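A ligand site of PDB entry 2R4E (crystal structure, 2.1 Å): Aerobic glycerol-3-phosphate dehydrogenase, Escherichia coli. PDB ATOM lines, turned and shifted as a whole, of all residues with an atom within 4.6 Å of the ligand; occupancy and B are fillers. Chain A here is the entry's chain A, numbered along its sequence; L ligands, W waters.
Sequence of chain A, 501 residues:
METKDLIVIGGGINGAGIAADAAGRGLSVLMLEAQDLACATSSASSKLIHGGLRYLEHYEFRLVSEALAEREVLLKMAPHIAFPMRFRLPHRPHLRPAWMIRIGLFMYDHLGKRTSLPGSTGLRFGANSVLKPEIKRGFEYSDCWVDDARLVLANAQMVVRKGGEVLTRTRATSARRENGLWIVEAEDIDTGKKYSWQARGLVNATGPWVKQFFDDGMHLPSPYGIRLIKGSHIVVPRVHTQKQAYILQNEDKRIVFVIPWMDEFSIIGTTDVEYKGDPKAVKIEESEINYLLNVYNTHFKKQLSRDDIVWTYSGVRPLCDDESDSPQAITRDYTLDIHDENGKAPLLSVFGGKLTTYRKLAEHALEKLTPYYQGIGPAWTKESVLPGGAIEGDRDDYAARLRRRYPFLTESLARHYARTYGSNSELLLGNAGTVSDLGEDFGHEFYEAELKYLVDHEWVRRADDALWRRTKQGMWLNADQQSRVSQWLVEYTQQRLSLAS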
ATOM      1  N   ARG A  54      15.190 -10.594 -10.724  1.00  0.00           N
ATOM      2  CA  ARG A  54      15.436 -10.768  -9.260  1.00  0.00           C
ATOM      3  C   ARG A  54      16.109  -9.568  -8.540  1.00  0.00           C
ATOM      4  O   ARG A  54      15.952  -9.453  -7.317  1.00  0.00           O
ATOM      5  CB  ARG A  54      16.222 -12.068  -8.990  1.00  0.00           C
ATOM      6  CG  ARG A  54      17.689 -11.991  -9.359  1.00  0.00           C
ATOM      7  CD  ARG A  54      18.330 -13.363  -9.083  1.00  0.00           C
ATOM      8  NE  ARG A  54      19.746 -13.231  -8.780  1.00  0.00           N
ATOM      9  CZ  ARG A  54      20.269 -13.006  -7.573  1.00  0.00           C
ATOM     10  NH1 ARG A  54      19.480 -12.853  -6.500  1.00  0.00           N
ATOM     11  NH2 ARG A  54      21.590 -12.934  -7.439  1.00  0.00           N
ATOM     12  N   TYR A  55      16.875  -8.746  -9.276  1.00  0.00           N
ATOM     13  CA  TYR A  55      17.575  -7.575  -8.737  1.00  0.00           C
ATOM     14  C   TYR A  55      16.660  -6.388  -8.362  1.00  0.00           C
ATOM     15  O   TYR A  55      17.013  -5.576  -7.524  1.00  0.00           O
ATOM     16  CB  TYR A  55      18.713  -7.057  -9.637  1.00  0.00           C
ATOM     17  CG  TYR A  55      19.626  -8.120 -10.222  1.00  0.00           C
ATOM     18  CD1 TYR A  55      19.984  -9.276  -9.477  1.00  0.00           C
ATOM     19  CD2 TYR A  55      20.162  -7.959 -11.505  1.00  0.00           C
ATOM     20  CE1 TYR A  55      20.820 -10.260 -10.038  1.00  0.00           C
ATOM     21  CE2 TYR A  55      20.979  -8.923 -12.059  1.00  0.00           C
ATOM     22  CZ  TYR A  55      21.309 -10.060 -11.331  1.00  0.00           C
ATOM     23  OH  TYR A  55      22.129 -11.001 -11.919  1.00  0.00           O
ATOM     24  N   ARG A 254      16.099 -17.682  -4.144  1.00  0.00           N
ATOM     25  CA  ARG A 254      16.820 -17.623  -5.431  1.00  0.00           C
ATOM     26  C   ARG A 254      15.887 -18.115  -6.544  1.00  0.00           C
ATOM     27  O   ARG A 254      14.855 -18.722  -6.260  1.00  0.00           O
ATOM     28  CB  ARG A 254      18.127 -18.418  -5.381  1.00  0.00           C
ATOM     29  CG  ARG A 254      19.123 -17.911  -4.311  1.00  0.00           C
ATOM     30  CD  ARG A 254      20.454 -18.681  -4.497  1.00  0.00           C
ATOM     31  NE  ARG A 254      21.042 -18.352  -5.831  1.00  0.00           N
ATOM     32  CZ  ARG A 254      21.053 -19.148  -6.915  1.00  0.00           C
ATOM     33  NH1 ARG A 254      21.646 -18.706  -8.013  1.00  0.00           N
ATOM     34  NH2 ARG A 254      20.475 -20.364  -6.959  1.00  0.00           N
ATOM     35  N   ILE A 255      16.258 -17.823  -7.789  1.00  0.00           N
ATOM     36  CA  ILE A 255      15.557 -18.311  -8.938  1.00  0.00           C
ATOM     37  C   ILE A 255      16.529 -19.220  -9.706  1.00  0.00           C
ATOM     38  O   ILE A 255      17.749 -19.051  -9.650  1.00  0.00           O
ATOM     39  CB  ILE A 255      14.946 -17.124  -9.796  1.00  0.00           C
ATOM     40  CG1 ILE A 255      15.973 -16.031 -10.034  1.00  0.00           C
ATOM     41  CG2 ILE A 255      13.605 -16.515  -9.189  1.00  0.00           C
ATOM     42  CD1 ILE A 255      16.767 -16.183 -11.418  1.00  0.00           C
ATOM     43  N   VAL A 256      15.983 -20.236 -10.358  1.00  0.00           N
ATOM     44  CA  VAL A 256      16.790 -21.180 -11.077  1.00  0.00           C
ATOM     45  C   VAL A 256      16.124 -21.271 -12.479  1.00  0.00           C
ATOM     46  O   VAL A 256      14.922 -21.357 -12.589  1.00  0.00           O
ATOM     47  CB  VAL A 256      16.836 -22.534 -10.345  1.00  0.00           C
ATOM     48  CG1 VAL A 256      17.363 -23.612 -11.243  1.00  0.00           C
ATOM     49  CG2 VAL A 256      17.742 -22.413  -9.096  1.00  0.00           C
ATOM     50  N   PHE A 257      16.955 -21.196 -13.538  1.00  0.00           N
ATOM     51  CA  PHE A 257      16.478 -21.296 -14.908  1.00  0.00           C
ATOM     52  C   PHE A 257      16.508 -22.703 -15.463  1.00  0.00           C
ATOM     53  O   PHE A 257      17.321 -23.539 -15.036  1.00  0.00           O
ATOM     54  CB  PHE A 257      17.345 -20.419 -15.798  1.00  0.00           C
ATOM     55  CG  PHE A 257      17.309 -18.959 -15.438  1.00  0.00           C
ATOM     56  CD1 PHE A 257      16.204 -18.201 -15.745  1.00  0.00           C
ATOM     57  CD2 PHE A 257      18.429 -18.319 -14.866  1.00  0.00           C
ATOM     58  CE1 PHE A 257      16.176 -16.839 -15.464  1.00  0.00           C
ATOM     59  CE2 PHE A 257      18.421 -16.955 -14.594  1.00  0.00           C
ATOM     60  CZ  PHE A 257      17.284 -16.215 -14.878  1.00  0.00           C
ATOM     61  N   GLY A 269      20.425 -24.061 -14.333  1.00  0.00           N
ATOM     62  CA  GLY A 269      21.338 -23.391 -13.400  1.00  0.00           C
ATOM     63  C   GLY A 269      20.599 -22.129 -12.877  1.00  0.00           C
ATOM     64  O   GLY A 269      19.629 -21.715 -13.444  1.00  0.00           O
ATOM     65  N   THR A 270      21.169 -21.440 -11.877  1.00  0.00           N
ATOM     66  CA  THR A 270      22.513 -21.696 -11.393  1.00  0.00           C
ATOM     67  C   THR A 270      22.531 -21.567  -9.831  1.00  0.00           C
ATOM     68  O   THR A 270      21.442 -21.622  -9.191  1.00  0.00           O
ATOM     69  CB  THR A 270      23.555 -20.772 -12.114  1.00  0.00           C
ATOM     70  OG1 THR A 270      24.845 -21.159 -11.674  1.00  0.00           O
ATOM     71  CG2 THR A 270      23.390 -19.307 -11.782  1.00  0.00           C
ATOM     72  N   ASP A 272      24.937 -20.109  -6.066  1.00  0.00           N
ATOM     73  CA  ASP A 272      25.627 -18.922  -5.510  1.00  0.00           C
ATOM     74  C   ASP A 272      26.458 -19.490  -4.358  1.00  0.00           C
ATOM     75  O   ASP A 272      25.977 -19.561  -3.261  1.00  0.00           O
ATOM     76  CB  ASP A 272      24.577 -17.972  -4.925  1.00  0.00           C
ATOM     77  CG  ASP A 272      24.246 -16.833  -5.824  1.00  0.00           C
ATOM     78  OD1 ASP A 272      25.205 -16.192  -6.218  1.00  0.00           O
ATOM     79  OD2 ASP A 272      23.033 -16.552  -6.105  1.00  0.00           O
ATOM     80  N   ARG A 317      31.729 -15.797 -10.387  1.00  0.00           N
ATOM     81  CA  ARG A 317      31.401 -14.370 -10.640  1.00  0.00           C
ATOM     82  C   ARG A 317      32.407 -13.498  -9.934  1.00  0.00           C
ATOM     83  O   ARG A 317      32.595 -13.664  -8.708  1.00  0.00           O
ATOM     84  CB  ARG A 317      30.012 -14.012 -10.154  1.00  0.00           C
ATOM     85  CG  ARG A 317      28.909 -14.786 -10.797  1.00  0.00           C
ATOM     86  CD  ARG A 317      27.662 -14.610  -9.963  1.00  0.00           C
ATOM     87  NE  ARG A 317      26.491 -15.423 -10.304  1.00  0.00           N
ATOM     88  CZ  ARG A 317      26.196 -16.643  -9.803  1.00  0.00           C
ATOM     89  NH1 ARG A 317      27.029 -17.332  -9.007  1.00  0.00           N
ATOM     90  NH2 ARG A 317      25.026 -17.192 -10.076  1.00  0.00           N
ATOM     91  N   ARG A 332      25.257  -7.110  -8.613  1.00  0.00           N
ATOM     92  CA  ARG A 332      25.751  -7.548  -9.923  1.00  0.00           C
ATOM     93  C   ARG A 332      26.023  -6.369 -10.816  1.00  0.00           C
ATOM     94  O   ARG A 332      26.316  -6.531 -12.015  1.00  0.00           O
ATOM     95  CB  ARG A 332      24.723  -8.438 -10.605  1.00  0.00           C
ATOM     96  CG  ARG A 332      24.915  -9.960 -10.344  1.00  0.00           C
ATOM     97  CD  ARG A 332      24.686 -10.404  -8.911  1.00  0.00           C
ATOM     98  NE  ARG A 332      24.672 -11.842  -8.848  1.00  0.00           N
ATOM     99  CZ  ARG A 332      24.715 -12.556  -7.744  1.00  0.00           C
ATOM    100  NH1 ARG A 332      24.780 -11.937  -6.570  1.00  0.00           N
ATOM    101  NH2 ARG A 332      24.634 -13.896  -7.820  1.00  0.00           N
ATOM    102  N   LYS A 354      28.278  -7.865 -15.737  1.00  0.00           N
ATOM    103  CA  LYS A 354      27.666  -9.010 -16.410  1.00  0.00           C
ATOM    104  C   LYS A 354      27.772  -8.872 -17.927  1.00  0.00           C
ATOM    105  O   LYS A 354      27.921  -7.766 -18.450  1.00  0.00           O
ATOM    106  CB  LYS A 354      26.203  -9.155 -16.004  1.00  0.00           C
ATOM    107  CG  LYS A 354      25.961  -9.048 -14.500  1.00  0.00           C
ATOM    108  CD  LYS A 354      24.484  -8.998 -14.181  1.00  0.00           C
ATOM    109  CE  LYS A 354      23.658  -9.682 -15.253  1.00  0.00           C
ATOM    110  NZ  LYS A 354      23.050 -10.958 -14.774  1.00  0.00           N
HETATM  111  P1  LIG L   1      22.931 -14.312 -10.848  1.00  0.00           P
HETATM  112  O1  LIG L   1      21.866 -13.342 -11.124  1.00  0.00           O
HETATM  113  O2  LIG L   1      24.382 -13.692 -11.096  1.00  0.00           O
HETATM  114  O3  LIG L   1      22.879 -15.780 -11.067  1.00  0.00           O
HETATM  115  O4  LIG L   1      22.349 -14.710  -9.336  1.00  0.00           O
HETATM  116  C1  LIG L   1      21.689 -15.936  -8.757  1.00  0.00           C
HETATM  117  C2  LIG L   1      20.267 -16.513  -9.241  1.00  0.00           C
HETATM  118  O5  LIG L   1      19.197 -16.471  -8.466  1.00  0.00           O
HETATM  119  C3  LIG L   1      20.239 -17.250 -10.671  1.00  0.00           C
HETATM  120  O6  LIG L   1      20.211 -18.779 -10.622  1.00  0.00           O
HETATM  121  O   HOH W   1      22.491 -16.564 -14.128  1.00  0.00           O
HETATM  122  O   HOH W   2      25.547 -12.254 -13.252  1.00  0.00           O
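An oxygen (O6) of the ligand lies within hydrogen-bond range of the backbone carbonyl oxygen (O) of Ile 255 (2.7 Å).
An oxygen (O2) of the ligand is in salt-bridge range of the guanidinium group (NE) of Arg 332 (2.9 Å).
O6 of the ligand lies close to NH1 of Arg 254 (3.0 Å).
The backbone NH of Thr 270 sits at hydrogen-bond distance from an oxygen (O6) of the ligand (3.1 Å).
The guanidinium group (NH2) of Arg 317 is in salt-bridge range of an oxygen (O3) of the ligand (2.8 Å).
O1 of the ligand is in hydrogen-bond range of OH of Tyr 55 (2.5 Å).
O of Thr 270 is in hydrogen-bond range of O6 of the ligand (3.4 Å).
An oxygen (O5) of the ligand lies within hydrogen-bond range of the backbone NH (N) of Ile 255.
An oxygen (O1) of the ligand lies within salt-bridge range of the guanidinium group of Arg 54 (3.2 Å).
The side-chain carboxylate (OD1) of Asp 272 lies within salt-bridge range of the guanidinium group (NH2) of Arg 332 (2.9 Å).
The guanidinium group (NH1) of Arg 317 lies within salt-bridge range of the side-chain carboxylate (OD1) of Asp 272, at 3.5 Å.
The guanidinium group (NH2) of Arg 254 is in hydrogen-bond range of the backbone carbonyl oxygen (O) of Thr 270 (2.7 Å).
NZ of Lys 354 is in hydrogen-bond range of OH of Tyr 55.
The guanidinium group (NE) of Arg 254 lies within salt-bridge range of the side-chain carboxylate (OD2) of Asp 272, at 2.7 Å.
OD2 of Asp 272 touches C1 of the ligand, 3.0 Å away.
Hydrophobic or aromatic side chains within 4 Å of the ligand: Tyr 55 and Ile 255.
Eight residues have an atom within 4 Å of the ligand: Arg 54, Tyr 55, Arg 254, Ile 255, Thr 270, Asp 272, Arg 317 and Arg 332.
Water W2 lies within hydrogen-bond range of an oxygen (O2) of the ligand (2.8 Å) and the side-chain amino group of Lys 354 (3.2 Å).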
